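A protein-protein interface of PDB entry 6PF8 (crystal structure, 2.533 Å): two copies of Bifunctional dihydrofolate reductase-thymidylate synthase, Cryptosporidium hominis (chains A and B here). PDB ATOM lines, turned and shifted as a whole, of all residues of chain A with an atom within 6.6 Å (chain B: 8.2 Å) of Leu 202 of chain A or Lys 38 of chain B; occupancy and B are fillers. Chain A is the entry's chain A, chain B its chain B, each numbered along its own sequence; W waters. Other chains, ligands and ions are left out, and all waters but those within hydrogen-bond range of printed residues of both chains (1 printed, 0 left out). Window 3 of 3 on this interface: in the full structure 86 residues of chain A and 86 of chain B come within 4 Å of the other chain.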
ATOM      1  N   ASP A 197      -7.623 -36.169  13.916  1.00  0.00           N
ATOM      2  CA  ASP A 197      -9.081 -36.179  13.843  1.00  0.00           C
ATOM      3  C   ASP A 197      -9.615 -34.888  13.234  1.00  0.00           C
ATOM      4  O   ASP A 197     -10.607 -34.905  12.497  1.00  0.00           O
ATOM      5  CB  ASP A 197      -9.673 -36.410  15.232  1.00  0.00           C
ATOM      6  CG  ASP A 197      -9.199 -37.709  15.860  1.00  0.00           C
ATOM      7  OD1 ASP A 197      -7.971 -37.888  16.001  1.00  0.00           O
ATOM      8  OD2 ASP A 197     -10.050 -38.551  16.215  1.00  0.00           O
ATOM      9  N   ASP A 198      -8.966 -33.757  13.526  1.00  0.00           N
ATOM     10  CA  ASP A 198      -9.397 -32.488  12.946  1.00  0.00           C
ATOM     11  C   ASP A 198      -9.153 -32.458  11.443  1.00  0.00           C
ATOM     12  O   ASP A 198     -10.003 -31.984  10.680  1.00  0.00           O
ATOM     13  CB  ASP A 198      -8.677 -31.322  13.627  1.00  0.00           C
ATOM     14  CG  ASP A 198      -9.167 -31.074  15.042  1.00  0.00           C
ATOM     15  OD1 ASP A 198     -10.132 -31.743  15.470  1.00  0.00           O
ATOM     16  OD2 ASP A 198      -8.581 -30.211  15.730  1.00  0.00           O
ATOM     17  N   THR A 199      -7.995 -32.952  11.001  1.00  0.00           N
ATOM     18  CA  THR A 199      -7.698 -32.978   9.573  1.00  0.00           C
ATOM     19  C   THR A 199      -8.686 -33.857   8.817  1.00  0.00           C
ATOM     20  O   THR A 199      -9.151 -33.490   7.730  1.00  0.00           O
ATOM     21  CB  THR A 199      -6.265 -33.460   9.354  1.00  0.00           C
ATOM     22  OG1 THR A 199      -5.355 -32.518   9.935  1.00  0.00           O
ATOM     23  CG2 THR A 199      -5.963 -33.611   7.870  1.00  0.00           C
ATOM     24  N   VAL A 200      -9.038 -35.013   9.386  1.00  0.00           N
ATOM     25  CA  VAL A 200     -10.003 -35.895   8.738  1.00  0.00           C
ATOM     26  C   VAL A 200     -11.376 -35.237   8.683  1.00  0.00           C
ATOM     27  O   VAL A 200     -12.094 -35.352   7.681  1.00  0.00           O
ATOM     28  CB  VAL A 200     -10.049 -37.252   9.465  1.00  0.00           C
ATOM     29  CG1 VAL A 200     -11.154 -38.135   8.897  1.00  0.00           C
ATOM     30  CG2 VAL A 200      -8.704 -37.945   9.358  1.00  0.00           C
ATOM     31  N   ASP A 201     -11.757 -34.525   9.746  1.00  0.00           N
ATOM     32  CA  ASP A 201     -13.031 -33.810   9.743  1.00  0.00           C
ATOM     33  C   ASP A 201     -13.046 -32.721   8.678  1.00  0.00           C
ATOM     34  O   ASP A 201     -14.020 -32.582   7.929  1.00  0.00           O
ATOM     35  CB  ASP A 201     -13.298 -33.209  11.124  1.00  0.00           C
ATOM     36  CG  ASP A 201     -13.605 -34.259  12.171  1.00  0.00           C
ATOM     37  OD1 ASP A 201     -14.112 -35.341  11.805  1.00  0.00           O
ATOM     38  OD2 ASP A 201     -13.337 -34.000  13.363  1.00  0.00           O
ATOM     39  N   LEU A 202     -11.969 -31.933   8.600  1.00  0.00           N
ATOM     40  CA  LEU A 202     -11.902 -30.869   7.603  1.00  0.00           C
ATOM     41  C   LEU A 202     -11.922 -31.434   6.189  1.00  0.00           C
ATOM     42  O   LEU A 202     -12.583 -30.880   5.302  1.00  0.00           O
ATOM     43  CB  LEU A 202     -10.655 -30.016   7.825  1.00  0.00           C
ATOM     44  CG  LEU A 202     -10.612 -29.233   9.139  1.00  0.00           C
ATOM     45  CD1 LEU A 202      -9.293 -28.492   9.278  1.00  0.00           C
ATOM     46  CD2 LEU A 202     -11.785 -28.268   9.227  1.00  0.00           C
ATOM     47  N   LEU A 203     -11.206 -32.538   5.958  1.00  0.00           N
ATOM     48  CA  LEU A 203     -11.252 -33.181   4.650  1.00  0.00           C
ATOM     49  C   LEU A 203     -12.644 -33.713   4.339  1.00  0.00           C
ATOM     50  O   LEU A 203     -13.060 -33.720   3.175  1.00  0.00           O
ATOM     51  CB  LEU A 203     -10.223 -34.308   4.576  1.00  0.00           C
ATOM     52  CG  LEU A 203      -8.769 -33.855   4.452  1.00  0.00           C
ATOM     53  CD1 LEU A 203      -7.830 -35.047   4.512  1.00  0.00           C
ATOM     54  CD2 LEU A 203      -8.573 -33.072   3.154  1.00  0.00           C
ATOM     55  N   GLY A 204     -13.380 -34.156   5.362  1.00  0.00           N
ATOM     56  CA  GLY A 204     -14.744 -34.599   5.152  1.00  0.00           C
ATOM     57  C   GLY A 204     -15.722 -33.474   4.886  1.00  0.00           C
ATOM     58  O   GLY A 204     -16.807 -33.724   4.354  1.00  0.00           O
ATOM     59  N   GLU A 205     -15.367 -32.241   5.249  1.00  0.00           N
ATOM     60  CA  GLU A 205     -16.225 -31.104   4.933  1.00  0.00           C
ATOM     61  C   GLU A 205     -15.986 -30.615   3.511  1.00  0.00           C
ATOM     62  O   GLU A 205     -16.933 -30.234   2.816  1.00  0.00           O
ATOM     63  CB  GLU A 205     -15.988 -29.972   5.932  1.00  0.00           C
ATOM     64  CG  GLU A 205     -16.321 -30.338   7.372  1.00  0.00           C
ATOM     65  CD  GLU A 205     -15.870 -29.283   8.362  1.00  0.00           C
ATOM     66  OE1 GLU A 205     -15.422 -28.205   7.918  1.00  0.00           O
ATOM     67  OE2 GLU A 205     -15.961 -29.531   9.584  1.00  0.00           O
ATOM     68  N   ILE A 206     -14.731 -30.630   3.068  1.00  0.00           N
ATOM     69  CA  ILE A 206     -14.361 -30.229   1.715  1.00  0.00           C
ATOM     70  C   ILE A 206     -14.944 -31.214   0.713  1.00  0.00           C
ATOM     71  O   ILE A 206     -15.806 -30.855  -0.098  1.00  0.00           O
ATOM     72  CB  ILE A 206     -12.833 -30.131   1.580  1.00  0.00           C
ATOM     73  CG1 ILE A 206     -12.285 -29.092   2.561  1.00  0.00           C
ATOM     74  CG2 ILE A 206     -12.443 -29.801   0.145  1.00  0.00           C
ATOM     75  CD1 ILE A 206     -10.787 -29.110   2.681  1.00  0.00           C
ATOM     76  N   PHE A 207     -14.472 -32.455   0.750  1.00  0.00           N
ATOM     77  CA  PHE A 207     -15.036 -33.507  -0.083  1.00  0.00           C
ATOM     78  C   PHE A 207     -16.268 -34.078   0.607  1.00  0.00           C
ATOM     79  O   PHE A 207     -16.237 -34.366   1.806  1.00  0.00           O
ATOM     80  CB  PHE A 207     -13.999 -34.604  -0.327  1.00  0.00           C
ATOM     81  CG  PHE A 207     -12.658 -34.091  -0.787  1.00  0.00           C
ATOM     82  CD1 PHE A 207     -12.392 -33.924  -2.137  1.00  0.00           C
ATOM     83  CD2 PHE A 207     -11.660 -33.787   0.129  1.00  0.00           C
ATOM     84  CE1 PHE A 207     -11.160 -33.459  -2.567  1.00  0.00           C
ATOM     85  CE2 PHE A 207     -10.424 -33.320  -0.294  1.00  0.00           C
ATOM     86  CZ  PHE A 207     -10.176 -33.157  -1.644  1.00  0.00           C
ATOM     87  N   GLU B  31      -9.729 -27.692  -4.174  1.00  0.00           N
ATOM     88  CA  GLU B  31      -9.901 -28.329  -2.872  1.00  0.00           C
ATOM     89  C   GLU B  31      -8.683 -28.134  -1.977  1.00  0.00           C
ATOM     90  O   GLU B  31      -8.816 -28.114  -0.748  1.00  0.00           O
ATOM     91  CB  GLU B  31     -10.198 -29.818  -3.050  1.00  0.00           C
ATOM     92  CG  GLU B  31     -11.544 -30.120  -3.701  1.00  0.00           C
ATOM     93  CD  GLU B  31     -11.497 -30.122  -5.224  1.00  0.00           C
ATOM     94  OE1 GLU B  31     -10.558 -29.545  -5.814  1.00  0.00           O
ATOM     95  OE2 GLU B  31     -12.402 -30.727  -5.833  1.00  0.00           O
ATOM     96  N   ASP B  32      -7.494 -27.984  -2.567  1.00  0.00           N
ATOM     97  CA  ASP B  32      -6.301 -27.750  -1.758  1.00  0.00           C
ATOM     98  C   ASP B  32      -6.313 -26.357  -1.141  1.00  0.00           C
ATOM     99  O   ASP B  32      -5.833 -26.166  -0.018  1.00  0.00           O
ATOM    100  CB  ASP B  32      -5.040 -27.947  -2.596  1.00  0.00           C
ATOM    101  CG  ASP B  32      -3.776 -27.605  -1.828  1.00  0.00           C
ATOM    102  OD1 ASP B  32      -3.492 -28.270  -0.807  1.00  0.00           O
ATOM    103  OD2 ASP B  32      -3.072 -26.660  -2.244  1.00  0.00           O
ATOM    104  N   LEU B  33      -6.839 -25.366  -1.862  1.00  0.00           N
ATOM    105  CA  LEU B  33      -6.953 -24.035  -1.278  1.00  0.00           C
ATOM    106  C   LEU B  33      -7.959 -24.024  -0.136  1.00  0.00           C
ATOM    107  O   LEU B  33      -7.747 -23.348   0.878  1.00  0.00           O
ATOM    108  CB  LEU B  33      -7.338 -23.017  -2.348  1.00  0.00           C
ATOM    109  CG  LEU B  33      -6.281 -22.770  -3.423  1.00  0.00           C
ATOM    110  CD1 LEU B  33      -6.714 -21.630  -4.336  1.00  0.00           C
ATOM    111  CD2 LEU B  33      -4.921 -22.486  -2.795  1.00  0.00           C
ATOM    112  N   LYS B  34      -9.059 -24.768  -0.279  1.00  0.00           N
ATOM    113  CA  LYS B  34     -10.011 -24.887   0.819  1.00  0.00           C
ATOM    114  C   LYS B  34      -9.380 -25.586   2.018  1.00  0.00           C
ATOM    115  O   LYS B  34      -9.649 -25.220   3.167  1.00  0.00           O
ATOM    116  CB  LYS B  34     -11.267 -25.628   0.358  1.00  0.00           C
ATOM    117  CG  LYS B  34     -12.013 -24.933  -0.769  1.00  0.00           C
ATOM    118  CD  LYS B  34     -13.376 -25.565  -1.009  1.00  0.00           C
ATOM    119  CE  LYS B  34     -14.062 -24.949  -2.218  1.00  0.00           C
ATOM    120  NZ  LYS B  34     -14.128 -23.461  -2.126  1.00  0.00           N
ATOM    121  N   PHE B  35      -8.529 -26.587   1.773  1.00  0.00           N
ATOM    122  CA  PHE B  35      -7.811 -27.226   2.872  1.00  0.00           C
ATOM    123  C   PHE B  35      -6.902 -26.231   3.575  1.00  0.00           C
ATOM    124  O   PHE B  35      -6.869 -26.166   4.809  1.00  0.00           O
ATOM    125  CB  PHE B  35      -7.004 -28.421   2.363  1.00  0.00           C
ATOM    126  CG  PHE B  35      -6.210 -29.113   3.438  1.00  0.00           C
ATOM    127  CD1 PHE B  35      -6.835 -29.966   4.335  1.00  0.00           C
ATOM    128  CD2 PHE B  35      -4.847 -28.904   3.560  1.00  0.00           C
ATOM    129  CE1 PHE B  35      -6.113 -30.602   5.328  1.00  0.00           C
ATOM    130  CE2 PHE B  35      -4.119 -29.537   4.552  1.00  0.00           C
ATOM    131  CZ  PHE B  35      -4.754 -30.387   5.438  1.00  0.00           C
ATOM    132  N   PHE B  36      -6.145 -25.449   2.800  1.00  0.00           N
ATOM    133  CA  PHE B  36      -5.318 -24.403   3.390  1.00  0.00           C
ATOM    134  C   PHE B  36      -6.164 -23.443   4.217  1.00  0.00           C
ATOM    135  O   PHE B  36      -5.767 -23.041   5.316  1.00  0.00           O
ATOM    136  CB  PHE B  36      -4.562 -23.652   2.291  1.00  0.00           C
ATOM    137  CG  PHE B  36      -3.762 -22.478   2.793  1.00  0.00           C
ATOM    138  CD1 PHE B  36      -2.431 -22.632   3.146  1.00  0.00           C
ATOM    139  CD2 PHE B  36      -4.339 -21.221   2.905  1.00  0.00           C
ATOM    140  CE1 PHE B  36      -1.694 -21.552   3.607  1.00  0.00           C
ATOM    141  CE2 PHE B  36      -3.610 -20.144   3.368  1.00  0.00           C
ATOM    142  CZ  PHE B  36      -2.286 -20.307   3.717  1.00  0.00           C
ATOM    143  N   SER B  37      -7.341 -23.076   3.706  1.00  0.00           N
ATOM    144  CA  SER B  37      -8.201 -22.137   4.420  1.00  0.00           C
ATOM    145  C   SER B  37      -8.722 -22.734   5.723  1.00  0.00           C
ATOM    146  O   SER B  37      -8.736 -22.061   6.760  1.00  0.00           O
ATOM    147  CB  SER B  37      -9.360 -21.705   3.523  1.00  0.00           C
ATOM    148  OG  SER B  37     -10.215 -20.798   4.195  1.00  0.00           O
ATOM    149  N   LYS B  38      -9.166 -23.992   5.690  1.00  0.00           N
ATOM    150  CA  LYS B  38      -9.751 -24.593   6.885  1.00  0.00           C
ATOM    151  C   LYS B  38      -8.693 -24.872   7.948  1.00  0.00           C
ATOM    152  O   LYS B  38      -8.951 -24.702   9.144  1.00  0.00           O
ATOM    153  CB  LYS B  38     -10.498 -25.875   6.510  1.00  0.00           C
ATOM    154  CG  LYS B  38     -11.646 -25.635   5.540  1.00  0.00           C
ATOM    155  CD  LYS B  38     -12.840 -26.522   5.827  1.00  0.00           C
ATOM    156  CE  LYS B  38     -14.058 -26.032   5.061  1.00  0.00           C
ATOM    157  NZ  LYS B  38     -15.313 -26.687   5.513  1.00  0.00           N
ATOM    158  N   ILE B  39      -7.491 -25.274   7.535  1.00  0.00           N
ATOM    159  CA  ILE B  39      -6.479 -25.639   8.521  1.00  0.00           C
ATOM    160  C   ILE B  39      -5.851 -24.400   9.159  1.00  0.00           C
ATOM    161  O   ILE B  39      -5.443 -24.444  10.326  1.00  0.00           O
ATOM    162  CB  ILE B  39      -5.420 -26.564   7.888  1.00  0.00           C
ATOM    163  CG1 ILE B  39      -4.698 -27.376   8.966  1.00  0.00           C
ATOM    164  CG2 ILE B  39      -4.408 -25.775   7.073  1.00  0.00           C
ATOM    165  CD1 ILE B  39      -5.584 -28.376   9.684  1.00  0.00           C
ATOM    166  N   THR B  40      -5.784 -23.275   8.439  1.00  0.00           N
ATOM    167  CA  THR B  40      -5.196 -22.064   9.001  1.00  0.00           C
ATOM    168  C   THR B  40      -6.205 -21.220   9.768  1.00  0.00           C
ATOM    169  O   THR B  40      -5.798 -20.376  10.575  1.00  0.00           O
ATOM    170  CB  THR B  40      -4.546 -21.207   7.904  1.00  0.00           C
ATOM    171  OG1 THR B  40      -5.516 -20.863   6.908  1.00  0.00           O
ATOM    172  CG2 THR B  40      -3.391 -21.958   7.242  1.00  0.00           C
ATOM    173  N   ASN B  41      -7.504 -21.430   9.543  1.00  0.00           N
ATOM    174  CA  ASN B  41      -8.535 -20.761  10.325  1.00  0.00           C
ATOM    175  C   ASN B  41      -8.917 -21.532  11.580  1.00  0.00           C
ATOM    176  O   ASN B  41      -9.518 -20.949  12.488  1.00  0.00           O
ATOM    177  CB  ASN B  41      -9.799 -20.554   9.480  1.00  0.00           C
ATOM    178  CG  ASN B  41      -9.748 -19.298   8.633  1.00  0.00           C
ATOM    179  OD1 ASN B  41      -9.471 -18.208   9.132  1.00  0.00           O
ATOM    180  ND2 ASN B  41     -10.025 -19.446   7.342  1.00  0.00           N
ATOM    181  N   ASN B  42      -8.567 -22.815  11.656  1.00  0.00           N
ATOM    182  CA  ASN B  42      -8.980 -23.662  12.767  1.00  0.00           C
ATOM    183  C   ASN B  42      -8.344 -23.178  14.067  1.00  0.00           C
ATOM    184  O   ASN B  42      -7.115 -23.096  14.174  1.00  0.00           O
ATOM    185  CB  ASN B  42      -8.597 -25.113  12.485  1.00  0.00           C
ATOM    186  CG  ASN B  42      -9.222 -26.086  13.467  1.00  0.00           C
ATOM    187  OD1 ASN B  42     -10.290 -25.826  14.024  1.00  0.00           O
ATOM    188  ND2 ASN B  42      -8.558 -27.215  13.687  1.00  0.00           N
ATOM    189  N   LYS B  43      -9.179 -22.866  15.054  1.00  0.00           N
ATOM    190  CA  LYS B  43      -8.695 -22.385  16.340  1.00  0.00           C
ATOM    191  C   LYS B  43      -9.743 -22.681  17.402  1.00  0.00           C
ATOM    192  O   LYS B  43     -10.903 -22.969  17.094  1.00  0.00           O
ATOM    193  CB  LYS B  43      -8.371 -20.887  16.295  1.00  0.00           C
ATOM    194  CG  LYS B  43      -9.551 -20.009  15.921  1.00  0.00           C
ATOM    195  CD  LYS B  43      -9.115 -18.574  15.673  1.00  0.00           C
ATOM    196  CE  LYS B  43     -10.290 -17.707  15.257  1.00  0.00           C
ATOM    197  NZ  LYS B  43     -11.240 -17.491  16.381  1.00  0.00           N
ATOM    198  N   ASN B  50      -5.146 -16.622  14.248  1.00  0.00           N
ATOM    199  CA  ASN B  50      -3.954 -17.352  13.848  1.00  0.00           C
ATOM    200  C   ASN B  50      -3.075 -16.474  12.963  1.00  0.00           C
ATOM    201  O   ASN B  50      -3.567 -15.627  12.213  1.00  0.00           O
ATOM    202  CB  ASN B  50      -4.321 -18.643  13.113  1.00  0.00           C
ATOM    203  CG  ASN B  50      -4.919 -19.690  14.038  1.00  0.00           C
ATOM    204  OD1 ASN B  50      -4.658 -19.694  15.243  1.00  0.00           O
ATOM    205  ND2 ASN B  50      -5.720 -20.588  13.479  1.00  0.00           N
ATOM    206  N   ARG B  70      -7.628 -13.860   9.699  1.00  0.00           N
ATOM    207  CA  ARG B  70      -6.264 -14.210  10.063  1.00  0.00           C
ATOM    208  C   ARG B  70      -5.357 -12.995   9.942  1.00  0.00           C
ATOM    209  O   ARG B  70      -5.703 -11.991   9.313  1.00  0.00           O
ATOM    210  CB  ARG B  70      -5.737 -15.358   9.194  1.00  0.00           C
ATOM    211  CG  ARG B  70      -6.322 -16.712   9.556  1.00  0.00           C
ATOM    212  CD  ARG B  70      -6.413 -17.611   8.340  1.00  0.00           C
ATOM    213  NE  ARG B  70      -7.396 -17.107   7.387  1.00  0.00           N
ATOM    214  CZ  ARG B  70      -7.585 -17.611   6.172  1.00  0.00           C
ATOM    215  NH1 ARG B  70      -6.853 -18.636   5.757  1.00  0.00           N
ATOM    216  NH2 ARG B  70      -8.503 -17.084   5.371  1.00  0.00           N
ATOM    217  N   PHE B 111       1.402 -20.441  11.579  1.00  0.00           N
ATOM    218  CA  PHE B 111       1.532 -21.245  10.368  1.00  0.00           C
ATOM    219  C   PHE B 111       2.586 -20.630   9.461  1.00  0.00           C
ATOM    220  O   PHE B 111       2.487 -19.454   9.098  1.00  0.00           O
ATOM    221  CB  PHE B 111       0.193 -21.359   9.631  1.00  0.00           C
ATOM    222  CG  PHE B 111      -0.859 -22.109  10.395  1.00  0.00           C
ATOM    223  CD1 PHE B 111      -1.762 -21.435  11.201  1.00  0.00           C
ATOM    224  CD2 PHE B 111      -0.945 -23.490  10.306  1.00  0.00           C
ATOM    225  CE1 PHE B 111      -2.732 -22.125  11.908  1.00  0.00           C
ATOM    226  CE2 PHE B 111      -1.911 -24.185  11.010  1.00  0.00           C
ATOM    227  CZ  PHE B 111      -2.806 -23.501  11.812  1.00  0.00           C
ATOM    228  N   TYR B 132       1.979 -29.964   7.475  1.00  0.00           N
ATOM    229  CA  TYR B 132       0.816 -30.349   6.682  1.00  0.00           C
ATOM    230  C   TYR B 132       1.232 -30.335   5.216  1.00  0.00           C
ATOM    231  O   TYR B 132       1.487 -29.267   4.649  1.00  0.00           O
ATOM    232  CB  TYR B 132      -0.364 -29.408   6.924  1.00  0.00           C
ATOM    233  CG  TYR B 132      -0.925 -29.436   8.330  1.00  0.00           C
ATOM    234  CD1 TYR B 132      -1.874 -30.380   8.704  1.00  0.00           C
ATOM    235  CD2 TYR B 132      -0.529 -28.497   9.275  1.00  0.00           C
ATOM    236  CE1 TYR B 132      -2.395 -30.400   9.985  1.00  0.00           C
ATOM    237  CE2 TYR B 132      -1.045 -28.508  10.556  1.00  0.00           C
ATOM    238  CZ  TYR B 132      -1.978 -29.462  10.906  1.00  0.00           C
ATOM    239  OH  TYR B 132      -2.494 -29.476  12.182  1.00  0.00           O
HETATM  240  O   HOH W   1      -5.293 -30.395  12.488  1.00  0.00           O
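OE1 of Glu 205 of chain A is in salt-bridge range of NZ of Lys 38 of chain B, at 2.8 Å.
The side-chain amide nitrogen (ND2) of Asn 50 of chain B lies within hydrogen-bond range of the backbone carbonyl oxygen (O) of Asn 42 of chain B.
Among the printed residues, merely in contact across the chains: Ile 206 of chain A with Phe 35 of chain B, Phe 207 of chain A with Glu 31 of chain B, Asp 198 of chain A with Asn 42 of chain B, Thr 199 of chain A with Tyr 132 of chain B, Leu 202 of chain A with Ile 39 of chain B, Leu 203 of chain A with Phe 35 of chain B, Leu 202 of chain A with Lys 38 of chain B, Ile 206 of chain A with Lys 34 of chain B, Ile 206 of chain A with Glu 31 of chain B and Thr 199 of chain A with Phe 35 of chain B.
Of the printed residues of chain B, Leu 202 of chain A touches Lys 38 and Ile 39.
Of chain A, only Leu 202 (3.8 Å) and Glu 205 (2.8 Å) come within 4 Å of Lys 38 of chain B.
Printed residues of chain B within 4 Å of Glu 205 of chain A: Lys 38.
Of the printed residues of chain B, Thr 199 of chain A touches Phe 35 and Tyr 132.
Printed residues of chain B within 4 Å of Leu 203 of chain A: Phe 35.
Of the printed residues of chain A, Glu 31 of chain B touches Ile 206 (3.9 Å) and Phe 207 (3.5 Å).
Asp 32 of chain B touches none of the printed residues of chain A.
Asn 50 of chain B touches none of the printed residues of chain A.
Of the 11 printed residues of chain A, 7 touch a printed residue of chain B.
Hydrophobic or aromatic side chains of chain A within 4 Å of the printed part of chain B: Leu 202, Leu 203, Ile 206 and Phe 207.
Of the 17 printed residues of chain B, 7 touch a printed residue of chain A.
Among the printed residues, 11 pairs touch across the chains.
Among the printed residues, Asp or Glu carboxylates within 4 Å of a Lys or Arg side-chain nitrogen of the other chain: Glu 205 of chain A with Lys 38 of chain B.
No position is printed for both chains.
Water W1 bridges OH of Tyr 132 of chain B and OG1 of Thr 199 of chain A.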
